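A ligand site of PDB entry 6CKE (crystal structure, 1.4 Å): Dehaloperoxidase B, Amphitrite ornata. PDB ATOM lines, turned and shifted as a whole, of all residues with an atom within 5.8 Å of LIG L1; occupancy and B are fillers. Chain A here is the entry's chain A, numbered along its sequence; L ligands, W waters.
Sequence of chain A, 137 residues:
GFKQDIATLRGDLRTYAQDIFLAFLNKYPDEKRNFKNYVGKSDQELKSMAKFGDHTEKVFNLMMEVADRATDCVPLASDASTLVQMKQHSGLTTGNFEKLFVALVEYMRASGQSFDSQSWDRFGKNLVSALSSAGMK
A ring nitrogen (NE2) of His 55 sits at hydrogen-bond distance from an oxygen (O2) of LG2 L2 (2.6 Å).
A ring nitrogen (NE2) of His 89 binds an iron atom (FE1) of LIG L1, at 2.2 Å.
A ring nitrogen (ND1) of His 55 is in hydrogen-bond range of an oxygen (O1) of LIG L1.
CZ of Phe 24 touches C26 of LIG L1, 3.7 Å away.
Glu 31 touches LIG L1 (OE2 to C26, 3.3 Å).
O of Asn 34 touches C31 of LIG L1, 3.2 Å away.
Phe 35 touches LIG L1 (CZ to C4, 3.5 Å).
Lys 58 touches LIG L1 (CD to O2, 3.4 Å).
Val 59 touches LIG L1.
CG of Leu 62 touches C17 of LIG L1, 3.9 Å away.
Met 63 touches LIG L1.
Leu 83 touches LIG L1.
Met 86 touches LIG L1.
Gln 88 touches LIG L1.
Leu 92 touches LIG L1 (CD1 to C23, 3.6 Å).
O of Asn 96 touches C24 of LIG L1, at 3.5 Å.
Phe 97 touches LIG L1 (CE1 to C3, 3.3 Å).
Leu 100 touches LIG L1 (CD2 to C18, 3.99 Å).
CD2 of Leu 127 touches C19 of LIG L1 (3.7 Å).
Hydrophobic or aromatic side chains that line LIG L1: Phe 24, Phe 35, His 55, Val 59, Leu 62, Met 63, Leu 83, Met 86, His 89, Leu 92, Phe 97, Leu 100 and Leu 127.
Along chain A the residues within 4 Å of LIG L1 span positions 24 to 127.
The nearest printed residue that does not touch LIG L1 is Phe 101 (4.2 Å).
Water W6 bridges O3 of LIG L1 (2.6 Å) and OD1 of Asn 37 (3.2 Å).
Water W1 lies within hydrogen-bond range of the backbone carbonyl oxygen (O) of Asn 34 (2.8 Å) and an oxygen (O3) of LIG L1 (3.2 Å).
Water W2 bridges OH of Tyr 38 and O3 of LIG L1.
The backbone carbonyl oxygen of Leu 83 lies within hydrogen-bond range of a ring nitrogen (ND1) of His 89, 2.8 Å away.
ND2 of Asn 34 is in hydrogen-bond range of O of Glu 31 (3.1 Å).
The side-chain carboxylate of Glu 31 lies within hydrogen-bond range of the side-chain amide nitrogen of Asn 96 (2.8 Å).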
ATOM      1  N   PHE A  24      15.703  -3.701 -23.179  1.00  0.00           N
ATOM      2  CA  PHE A  24      14.647  -4.218 -24.056  1.00  0.00           C
ATOM      3  C   PHE A  24      13.692  -3.118 -24.513  1.00  0.00           C
ATOM      4  O   PHE A  24      13.397  -2.989 -25.710  1.00  0.00           O
ATOM      5  CB  PHE A  24      13.902  -5.321 -23.299  1.00  0.00           C
ATOM      6  CG  PHE A  24      12.621  -5.781 -23.943  1.00  0.00           C
ATOM      7  CD1 PHE A  24      12.629  -6.487 -25.145  1.00  0.00           C
ATOM      8  CD2 PHE A  24      11.417  -5.535 -23.320  1.00  0.00           C
ATOM      9  CE1 PHE A  24      11.449  -6.920 -25.718  1.00  0.00           C
ATOM     10  CE2 PHE A  24      10.236  -5.978 -23.883  1.00  0.00           C
ATOM     11  CZ  PHE A  24      10.249  -6.674 -25.085  1.00  0.00           C
ATOM     12  N   GLU A  31       7.373  -2.365 -28.104  1.00  0.00           N
ATOM     13  CA  GLU A  31       7.045  -3.358 -27.099  1.00  0.00           C
ATOM     14  C   GLU A  31       6.411  -2.740 -25.854  1.00  0.00           C
ATOM     15  O   GLU A  31       5.811  -3.461 -25.055  1.00  0.00           O
ATOM     16  CB  GLU A  31       8.284  -4.182 -26.742  1.00  0.00           C
ATOM     17  CG  GLU A  31       8.742  -5.101 -27.853  1.00  0.00           C
ATOM     18  CD  GLU A  31       7.770  -6.218 -28.111  1.00  0.00           C
ATOM     19  OE1 GLU A  31       7.372  -6.416 -29.287  1.00  0.00           O
ATOM     20  OE2 GLU A  31       7.387  -6.900 -27.144  1.00  0.00           O
ATOM     21  N   ASN A  34       2.671  -3.350 -24.500  1.00  0.00           N
ATOM     22  CA  ASN A  34       2.367  -4.330 -23.482  1.00  0.00           C
ATOM     23  C   ASN A  34       2.539  -3.784 -22.066  1.00  0.00           C
ATOM     24  O   ASN A  34       2.218  -4.497 -21.113  1.00  0.00           O
ATOM     25  CB  ASN A  34       3.294  -5.534 -23.627  1.00  0.00           C
ATOM     26  CG  ASN A  34       3.220  -6.177 -24.999  1.00  0.00           C
ATOM     27  OD1 ASN A  34       2.223  -6.802 -25.339  1.00  0.00           O
ATOM     28  ND2 ASN A  34       4.278  -5.996 -25.801  1.00  0.00           N
ATOM     29  N   PHE A  35       3.078  -2.564 -21.921  1.00  0.00           N
ATOM     30  CA  PHE A  35       3.434  -2.009 -20.626  1.00  0.00           C
ATOM     31  C   PHE A  35       2.953  -0.568 -20.544  1.00  0.00           C
ATOM     32  O   PHE A  35       3.717   0.374 -20.337  1.00  0.00           O
ATOM     33  CB  PHE A  35       4.947  -2.108 -20.384  1.00  0.00           C
ATOM     34  CG  PHE A  35       5.464  -3.523 -20.380  1.00  0.00           C
ATOM     35  CD1 PHE A  35       6.038  -4.056 -21.524  1.00  0.00           C
ATOM     36  CD2 PHE A  35       5.319  -4.321 -19.261  1.00  0.00           C
ATOM     37  CE1 PHE A  35       6.503  -5.358 -21.528  1.00  0.00           C
ATOM     38  CE2 PHE A  35       5.771  -5.627 -19.261  1.00  0.00           C
ATOM     39  CZ  PHE A  35       6.361  -6.144 -20.388  1.00  0.00           C
ATOM     40  N   ASN A  37       1.621   1.202 -18.409  1.00  0.00           N
ATOM     41  CA  ASN A  37       1.867   1.967 -17.190  1.00  0.00           C
ATOM     42  C   ASN A  37       3.303   2.470 -17.059  1.00  0.00           C
ATOM     43  O   ASN A  37       3.621   3.139 -16.074  1.00  0.00           O
ATOM     44  CB  ASN A  37       1.480   1.151 -15.962  1.00  0.00           C
ATOM     45  CG  ASN A  37      -0.015   0.915 -15.866  1.00  0.00           C
ATOM     46  OD1 ASN A  37      -0.470  -0.221 -15.728  1.00  0.00           O
ATOM     47  ND2 ASN A  37      -0.785   1.992 -15.975  1.00  0.00           N
ATOM     48  N   TYR A  38       4.174   2.140 -18.023  1.00  0.00           N
ATOM     49  CA  TYR A  38       5.560   2.590 -17.983  1.00  0.00           C
ATOM     50  C   TYR A  38       5.869   3.592 -19.076  1.00  0.00           C
ATOM     51  O   TYR A  38       7.032   3.951 -19.269  1.00  0.00           O
ATOM     52  CB  TYR A  38       6.503   1.380 -18.018  1.00  0.00           C
ATOM     53  CG  TYR A  38       6.396   0.474 -16.811  1.00  0.00           C
ATOM     54  CD1 TYR A  38       6.209   1.007 -15.532  1.00  0.00           C
ATOM     55  CD2 TYR A  38       6.487  -0.909 -16.928  1.00  0.00           C
ATOM     56  CE1 TYR A  38       6.117   0.182 -14.423  1.00  0.00           C
ATOM     57  CE2 TYR A  38       6.388  -1.730 -15.816  1.00  0.00           C
ATOM     58  CZ  TYR A  38       6.207  -1.182 -14.570  1.00  0.00           C
ATOM     59  OH  TYR A  38       6.104  -1.989 -13.456  1.00  0.00           O
ATOM     60  N   ASP A  54       9.787  -3.666  -8.142  1.00  0.00           N
ATOM     61  CA  ASP A  54       9.108  -4.883  -7.703  1.00  0.00           C
ATOM     62  C   ASP A  54       8.761  -5.775  -8.891  1.00  0.00           C
ATOM     63  O   ASP A  54       8.987  -6.992  -8.857  1.00  0.00           O
ATOM     64  CB  ASP A  54       7.827  -4.518  -6.949  1.00  0.00           C
ATOM     65  CG  ASP A  54       8.096  -3.839  -5.615  1.00  0.00           C
ATOM     66  OD1 ASP A  54       7.162  -3.238  -5.051  1.00  0.00           O
ATOM     67  OD2 ASP A  54       9.244  -3.902  -5.132  1.00  0.00           O
ATOM     68  N   HIS A  55       8.191  -5.185  -9.942  1.00  0.00           N
ATOM     69  CA  HIS A  55       7.833  -5.938 -11.130  1.00  0.00           C
ATOM     70  C   HIS A  55       9.046  -6.591 -11.767  1.00  0.00           C
ATOM     71  O   HIS A  55       9.033  -7.799 -12.050  1.00  0.00           O
ATOM     72  CB  HIS A  55       7.169  -5.009 -12.139  1.00  0.00           C
ATOM     73  CG  HIS A  55       7.022  -5.616 -13.503  1.00  0.00           C
ATOM     74  ND1 HIS A  55       6.110  -6.608 -13.777  1.00  0.00           N
ATOM     75  CD2 HIS A  55       7.695  -5.384 -14.653  1.00  0.00           C
ATOM     76  CE1 HIS A  55       6.217  -6.957 -15.049  1.00  0.00           C
ATOM     77  NE2 HIS A  55       7.168  -6.228 -15.603  1.00  0.00           N
ATOM     78  N   LYS A  58      10.440  -9.549  -9.757  1.00  0.00           N
ATOM     79  CA  LYS A  58       9.628 -10.750  -9.801  1.00  0.00           C
ATOM     80  C   LYS A  58       9.756 -11.463 -11.143  1.00  0.00           C
ATOM     81  O   LYS A  58       9.838 -12.701 -11.206  1.00  0.00           O
ATOM     82  CB  LYS A  58       8.174 -10.402  -9.497  1.00  0.00           C
ATOM     83  CG  LYS A  58       7.935 -10.220  -8.004  1.00  0.00           C
ATOM     84  CD  LYS A  58       6.506  -9.839  -7.707  1.00  0.00           C
ATOM     85  CE  LYS A  58       6.123 -10.164  -6.274  1.00  0.00           C
ATOM     86  NZ  LYS A  58       7.096  -9.574  -5.308  1.00  0.00           N
ATOM     87  N   VAL A  59       9.777 -10.692 -12.239  1.00  0.00           N
ATOM     88  CA  VAL A  59       9.974 -11.290 -13.558  1.00  0.00           C
ATOM     89  C   VAL A  59      11.309 -12.008 -13.614  1.00  0.00           C
ATOM     90  O   VAL A  59      11.400 -13.161 -14.039  1.00  0.00           O
ATOM     91  CB  VAL A  59       9.890 -10.200 -14.642  1.00  0.00           C
ATOM     92  CG1 VAL A  59      10.311 -10.785 -15.988  1.00  0.00           C
ATOM     93  CG2 VAL A  59       8.494  -9.636 -14.721  1.00  0.00           C
ATOM     94  N   PHE A  60      12.377 -11.310 -13.221  1.00  0.00           N
ATOM     95  CA  PHE A  60      13.718 -11.857 -13.398  1.00  0.00           C
ATOM     96  C   PHE A  60      13.955 -13.038 -12.471  1.00  0.00           C
ATOM     97  O   PHE A  60      14.691 -13.966 -12.831  1.00  0.00           O
ATOM     98  CB  PHE A  60      14.745 -10.747 -13.171  1.00  0.00           C
ATOM     99  CG  PHE A  60      16.023 -10.892 -13.954  1.00  0.00           C
ATOM    100  CD1 PHE A  60      17.233 -10.668 -13.329  1.00  0.00           C
ATOM    101  CD2 PHE A  60      16.028 -11.245 -15.296  1.00  0.00           C
ATOM    102  CE1 PHE A  60      18.411 -10.776 -14.020  1.00  0.00           C
ATOM    103  CE2 PHE A  60      17.223 -11.353 -16.004  1.00  0.00           C
ATOM    104  CZ  PHE A  60      18.412 -11.116 -15.360  1.00  0.00           C
ATOM    105  N   LEU A  62      11.697 -15.329 -11.735  1.00  0.00           N
ATOM    106  CA  LEU A  62      11.172 -16.471 -12.467  1.00  0.00           C
ATOM    107  C   LEU A  62      12.058 -16.834 -13.652  1.00  0.00           C
ATOM    108  O   LEU A  62      12.278 -18.018 -13.922  1.00  0.00           O
ATOM    109  CB  LEU A  62       9.720 -16.224 -12.905  1.00  0.00           C
ATOM    110  CG  LEU A  62       9.087 -17.414 -13.632  1.00  0.00           C
ATOM    111  CD1 LEU A  62       9.129 -18.680 -12.787  1.00  0.00           C
ATOM    112  CD2 LEU A  62       7.650 -17.093 -14.039  1.00  0.00           C
ATOM    113  N   MET A  63      12.601 -15.840 -14.352  1.00  0.00           N
ATOM    114  CA  MET A  63      13.486 -16.181 -15.449  1.00  0.00           C
ATOM    115  C   MET A  63      14.699 -16.966 -14.964  1.00  0.00           C
ATOM    116  O   MET A  63      15.128 -17.927 -15.608  1.00  0.00           O
ATOM    117  CB  MET A  63      13.932 -14.924 -16.196  1.00  0.00           C
ATOM    118  CG  MET A  63      14.674 -15.264 -17.476  1.00  0.00           C
ATOM    119  SD  MET A  63      15.641 -13.931 -18.217  1.00  0.00           S
ATOM    120  CE  MET A  63      14.326 -12.844 -18.724  1.00  0.00           C
ATOM    121  N   VAL A  66      13.712 -20.590 -14.272  1.00  0.00           N
ATOM    122  CA  VAL A  66      13.608 -21.337 -15.521  1.00  0.00           C
ATOM    123  C   VAL A  66      14.994 -21.638 -16.064  1.00  0.00           C
ATOM    124  O   VAL A  66      15.275 -22.750 -16.513  1.00  0.00           O
ATOM    125  CB  VAL A  66      12.734 -20.577 -16.537  1.00  0.00           C
ATOM    126  CG1 VAL A  66      12.754 -21.252 -17.901  1.00  0.00           C
ATOM    127  CG2 VAL A  66      11.310 -20.437 -15.999  1.00  0.00           C
ATOM    128  N   LEU A  83       4.808 -20.205 -18.538  1.00  0.00           N
ATOM    129  CA  LEU A  83       4.917 -18.898 -19.180  1.00  0.00           C
ATOM    130  C   LEU A  83       3.826 -18.672 -20.220  1.00  0.00           C
ATOM    131  O   LEU A  83       3.358 -17.546 -20.384  1.00  0.00           O
ATOM    132  CB  LEU A  83       6.304 -18.729 -19.795  1.00  0.00           C
ATOM    133  CG  LEU A  83       7.440 -18.756 -18.782  1.00  0.00           C
ATOM    134  CD1 LEU A  83       8.747 -18.899 -19.523  1.00  0.00           C
ATOM    135  CD2 LEU A  83       7.428 -17.472 -17.964  1.00  0.00           C
ATOM    136  N   MET A  86       0.225 -18.118 -18.172  1.00  0.00           N
ATOM    137  CA  MET A  86       0.071 -16.980 -17.278  1.00  0.00           C
ATOM    138  C   MET A  86      -0.883 -15.963 -17.868  1.00  0.00           C
ATOM    139  O   MET A  86      -0.736 -15.548 -19.018  1.00  0.00           O
ATOM    140  CB  MET A  86       1.438 -16.333 -17.061  1.00  0.00           C
ATOM    141  CG  MET A  86       2.273 -16.992 -16.004  1.00  0.00           C
ATOM    142  SD  MET A  86       3.935 -16.291 -16.020  1.00  0.00           S
ATOM    143  CE  MET A  86       3.543 -14.575 -15.711  1.00  0.00           C
ATOM    144  N   GLN A  88      -1.075 -12.870 -17.357  1.00  0.00           N
ATOM    145  CA  GLN A  88      -0.378 -11.659 -17.772  1.00  0.00           C
ATOM    146  C   GLN A  88       0.251 -11.791 -19.159  1.00  0.00           C
ATOM    147  O   GLN A  88       0.596 -10.782 -19.775  1.00  0.00           O
ATOM    148  CB  GLN A  88       0.713 -11.287 -16.765  1.00  0.00           C
ATOM    149  CG  GLN A  88       0.260 -11.142 -15.313  1.00  0.00           C
ATOM    150  CD  GLN A  88       0.411 -12.419 -14.508  1.00  0.00           C
ATOM    151  OE1 GLN A  88       0.088 -13.513 -14.970  1.00  0.00           O
ATOM    152  NE2 GLN A  88       0.907 -12.274 -13.285  1.00  0.00           N
ATOM    153  N   HIS A  89       0.395 -13.021 -19.650  1.00  0.00           N
ATOM    154  CA  HIS A  89       0.996 -13.273 -20.948  1.00  0.00           C
ATOM    155  C   HIS A  89      -0.012 -13.615 -22.027  1.00  0.00           C
ATOM    156  O   HIS A  89       0.373 -14.093 -23.088  1.00  0.00           O
ATOM    157  CB  HIS A  89       2.028 -14.397 -20.841  1.00  0.00           C
ATOM    158  CG  HIS A  89       3.237 -14.029 -20.047  1.00  0.00           C
ATOM    159  ND1 HIS A  89       4.132 -14.967 -19.592  1.00  0.00           N
ATOM    160  CD2 HIS A  89       3.691 -12.825 -19.638  1.00  0.00           C
ATOM    161  CE1 HIS A  89       5.107 -14.348 -18.935  1.00  0.00           C
ATOM    162  NE2 HIS A  89       4.851 -13.057 -18.933  1.00  0.00           N
ATOM    163  N   LEU A  92       0.487 -12.499 -25.955  1.00  0.00           N
ATOM    164  CA  LEU A  92       1.880 -12.523 -26.390  1.00  0.00           C
ATOM    165  C   LEU A  92       2.107 -13.605 -27.446  1.00  0.00           C
ATOM    166  O   LEU A  92       1.404 -14.613 -27.499  1.00  0.00           O
ATOM    167  CB  LEU A  92       2.825 -12.786 -25.214  1.00  0.00           C
ATOM    168  CG  LEU A  92       2.769 -11.754 -24.084  1.00  0.00           C
ATOM    169  CD1 LEU A  92       3.804 -12.074 -23.029  1.00  0.00           C
ATOM    170  CD2 LEU A  92       2.957 -10.349 -24.622  1.00  0.00           C
ATOM    171  N   ASN A  96       7.719 -11.677 -29.073  1.00  0.00           N
ATOM    172  CA  ASN A  96       7.972 -10.843 -27.896  1.00  0.00           C
ATOM    173  C   ASN A  96       9.154 -11.375 -27.098  1.00  0.00           C
ATOM    174  O   ASN A  96       9.995 -10.613 -26.608  1.00  0.00           O
ATOM    175  CB  ASN A  96       6.727 -10.824 -27.014  1.00  0.00           C
ATOM    176  CG  ASN A  96       5.513 -10.208 -27.700  1.00  0.00           C
ATOM    177  OD1 ASN A  96       4.546 -10.902 -28.024  1.00  0.00           O
ATOM    178  ND2 ASN A  96       5.535  -8.892 -27.873  1.00  0.00           N
ATOM    179  N   PHE A  97       9.216 -12.690 -26.955  1.00  0.00           N
ATOM    180  CA  PHE A  97      10.302 -13.326 -26.202  1.00  0.00           C
ATOM    181  C   PHE A  97      11.597 -13.301 -26.983  1.00  0.00           C
ATOM    182  O   PHE A  97      12.676 -13.109 -26.407  1.00  0.00           O
ATOM    183  CB  PHE A  97       9.912 -14.767 -25.827  1.00  0.00           C
ATOM    184  CG  PHE A  97       8.839 -14.833 -24.788  1.00  0.00           C
ATOM    185  CD1 PHE A  97       9.153 -15.148 -23.481  1.00  0.00           C
ATOM    186  CD2 PHE A  97       7.507 -14.575 -25.120  1.00  0.00           C
ATOM    187  CE1 PHE A  97       8.163 -15.185 -22.514  1.00  0.00           C
ATOM    188  CE2 PHE A  97       6.521 -14.603 -24.154  1.00  0.00           C
ATOM    189  CZ  PHE A  97       6.840 -14.921 -22.859  1.00  0.00           C
ATOM    190  N   LEU A 100      13.085  -9.893 -26.387  1.00  0.00           N
ATOM    191  CA  LEU A 100      13.646  -9.808 -25.041  1.00  0.00           C
ATOM    192  C   LEU A 100      15.048 -10.412 -24.988  1.00  0.00           C
ATOM    193  O   LEU A 100      15.970  -9.805 -24.451  1.00  0.00           O
ATOM    194  CB  LEU A 100      12.725 -10.474 -24.037  1.00  0.00           C
ATOM    195  CG  LEU A 100      13.311 -10.617 -22.628  1.00  0.00           C
ATOM    196  CD1 LEU A 100      13.628  -9.238 -22.042  1.00  0.00           C
ATOM    197  CD2 LEU A 100      12.351 -11.376 -21.720  1.00  0.00           C
ATOM    198  N   PHE A 101      15.206 -11.602 -25.556  1.00  0.00           N
ATOM    199  CA  PHE A 101      16.510 -12.253 -25.448  1.00  0.00           C
ATOM    200  C   PHE A 101      17.563 -11.637 -26.354  1.00  0.00           C
ATOM    201  O   PHE A 101      18.736 -11.593 -25.981  1.00  0.00           O
ATOM    202  CB  PHE A 101      16.366 -13.778 -25.551  1.00  0.00           C
ATOM    203  CG  PHE A 101      15.873 -14.371 -24.283  1.00  0.00           C
ATOM    204  CD1 PHE A 101      14.512 -14.499 -24.049  1.00  0.00           C
ATOM    205  CD2 PHE A 101      16.760 -14.693 -23.270  1.00  0.00           C
ATOM    206  CE1 PHE A 101      14.049 -14.968 -22.839  1.00  0.00           C
ATOM    207  CE2 PHE A 101      16.288 -15.158 -22.057  1.00  0.00           C
ATOM    208  CZ  PHE A 101      14.941 -15.316 -21.840  1.00  0.00           C
ATOM    209  N   LEU A 127      14.113 -21.374 -25.566  1.00  0.00           N
ATOM    210  CA  LEU A 127      12.866 -21.001 -24.889  1.00  0.00           C
ATOM    211  C   LEU A 127      11.774 -20.660 -25.901  1.00  0.00           C
ATOM    212  O   LEU A 127      10.623 -21.060 -25.715  1.00  0.00           O
ATOM    213  CB  LEU A 127      13.109 -19.842 -23.925  1.00  0.00           C
ATOM    214  CG  LEU A 127      11.835 -19.340 -23.210  1.00  0.00           C
ATOM    215  CD1 LEU A 127      11.231 -20.390 -22.288  1.00  0.00           C
ATOM    216  CD2 LEU A 127      12.158 -18.052 -22.429  1.00  0.00           C
HETATM  217  C1  LIG L   1       4.171 -10.170 -15.953  1.00  0.00           C
HETATM  218  C2  LIG L   1       7.585 -13.591 -16.005  1.00  0.00           C
HETATM  219  C3  LIG L   1       8.562 -12.519 -20.632  1.00  0.00           C
HETATM  220  C4  LIG L   1       4.910  -9.352 -20.667  1.00  0.00           C
HETATM  221  C5  LIG L   1       5.048 -11.138 -15.536  1.00  0.00           C
HETATM  222  C6  LIG L   1       5.206 -11.641 -14.192  1.00  0.00           C
HETATM  223  C7  LIG L   1       6.158 -12.583 -14.195  1.00  0.00           C
HETATM  224  C8  LIG L   1       6.613 -12.719 -15.562  1.00  0.00           C
HETATM  225  C9  LIG L   1       6.670 -13.382 -12.985  1.00  0.00           C
HETATM  226  C10 LIG L   1       4.457 -11.102 -12.952  1.00  0.00           C
HETATM  227  C11 LIG L   1       5.288  -9.888 -12.541  1.00  0.00           C
HETATM  228  C12 LIG L   1       4.729  -9.073 -11.399  1.00  0.00           C
HETATM  229  O1  LIG L   1       4.627  -7.819 -11.562  1.00  0.00           O
HETATM  230  O2  LIG L   1       4.394  -9.678 -10.349  1.00  0.00           O
HETATM  231  C13 LIG L   1       8.156 -13.555 -17.245  1.00  0.00           C
HETATM  232  C14 LIG L   1       9.326 -14.314 -17.638  1.00  0.00           C
HETATM  233  C15 LIG L   1       9.608 -14.001 -18.918  1.00  0.00           C
HETATM  234  C16 LIG L   1       8.610 -13.057 -19.367  1.00  0.00           C
HETATM  235  C17 LIG L   1      10.073 -15.241 -16.659  1.00  0.00           C
HETATM  236  C18 LIG L   1      10.720 -14.508 -19.852  1.00  0.00           C
HETATM  237  C19 LIG L   1      11.280 -15.727 -19.726  1.00  0.00           C
HETATM  238  C20 LIG L   1       7.672 -11.556 -21.045  1.00  0.00           C
HETATM  239  C21 LIG L   1       7.675 -10.887 -22.322  1.00  0.00           C
HETATM  240  C22 LIG L   1       6.663 -10.019 -22.344  1.00  0.00           C
HETATM  241  C23 LIG L   1       6.003 -10.097 -21.063  1.00  0.00           C
HETATM  242  C24 LIG L   1       8.691 -11.224 -23.425  1.00  0.00           C
HETATM  243  C25 LIG L   1       6.215  -9.025 -23.439  1.00  0.00           C
HETATM  244  C26 LIG L   1       7.076  -8.504 -24.312  1.00  0.00           C
HETATM  245  C27 LIG L   1       4.400  -9.314 -19.402  1.00  0.00           C
HETATM  246  C28 LIG L   1       3.327  -8.441 -18.975  1.00  0.00           C
HETATM  247  C29 LIG L   1       3.105  -8.657 -17.670  1.00  0.00           C
HETATM  248  C30 LIG L   1       4.046  -9.662 -17.224  1.00  0.00           C
HETATM  249  C31 LIG L   1       2.581  -7.453 -19.909  1.00  0.00           C
HETATM  250  C32 LIG L   1       2.052  -7.950 -16.790  1.00  0.00           C
HETATM  251  C33 LIG L   1       2.643  -6.626 -16.317  1.00  0.00           C
HETATM  252  C34 LIG L   1       1.628  -5.858 -15.512  1.00  0.00           C
HETATM  253  O3  LIG L   1       1.449  -4.650 -15.809  1.00  0.00           O
HETATM  254  O4  LIG L   1       1.004  -6.441 -14.590  1.00  0.00           O
HETATM  255  N1  LIG L   1       5.918 -11.828 -16.359  1.00  0.00           N
HETATM  256  N2  LIG L   1       7.741 -12.808 -18.323  1.00  0.00           N
HETATM  257  N3  LIG L   1       6.625 -11.045 -20.285  1.00  0.00           N
HETATM  258  N4  LIG L   1       4.802 -10.043 -18.319  1.00  0.00           N
HETATM  259 FE1  LIG L   1       6.201 -11.489 -18.341  1.00  0.00          FE
HETATM  260  C1  LG2 L   2      10.178  -8.138 -18.753  1.00  0.00           C
HETATM  261  C2  LG2 L   2      11.499  -8.500 -18.678  1.00  0.00           C
HETATM  262  C3  LG2 L   2       9.608  -7.452 -17.709  1.00  0.00           C
HETATM  263  C4  LG2 L   2      10.343  -7.119 -16.585  1.00  0.00           C
HETATM  264  C5  LG2 L   2      12.242  -8.172 -17.557  1.00  0.00           C
HETATM  265  C6  LG2 L   2      11.672  -7.473 -16.502  1.00  0.00           C
HETATM  266  O1  LG2 L   2       9.331  -8.445 -19.834  1.00  0.00           O
HETATM  267 BR1  LG2 L   2      14.100  -8.687 -17.463  1.00  0.00          BR
HETATM  268  O2  LG2 L   2       8.266  -7.141 -17.831  1.00  0.00           O
HETATM  269  C7  LG2 L   2       9.829  -8.280 -21.127  1.00  0.00           C
HETATM  270  O   HOH W   1       0.712  -4.076 -18.846  1.00  0.00           O
HETATM  271  O   HOH W   2       3.969  -3.751 -13.750  1.00  0.00           O
HETATM  272  O   HOH W   3      -0.215  -5.996 -21.423  1.00  0.00           O
HETATM  273  O   HOH W   4       7.660  -9.920 -17.960  1.00  0.00           O
HETATM  274  O   HOH W   5       4.918  -6.448  -9.113  1.00  0.00           O
HETATM  275  O   HOH W   6       0.701  -2.777 -14.212  1.00  0.00           O
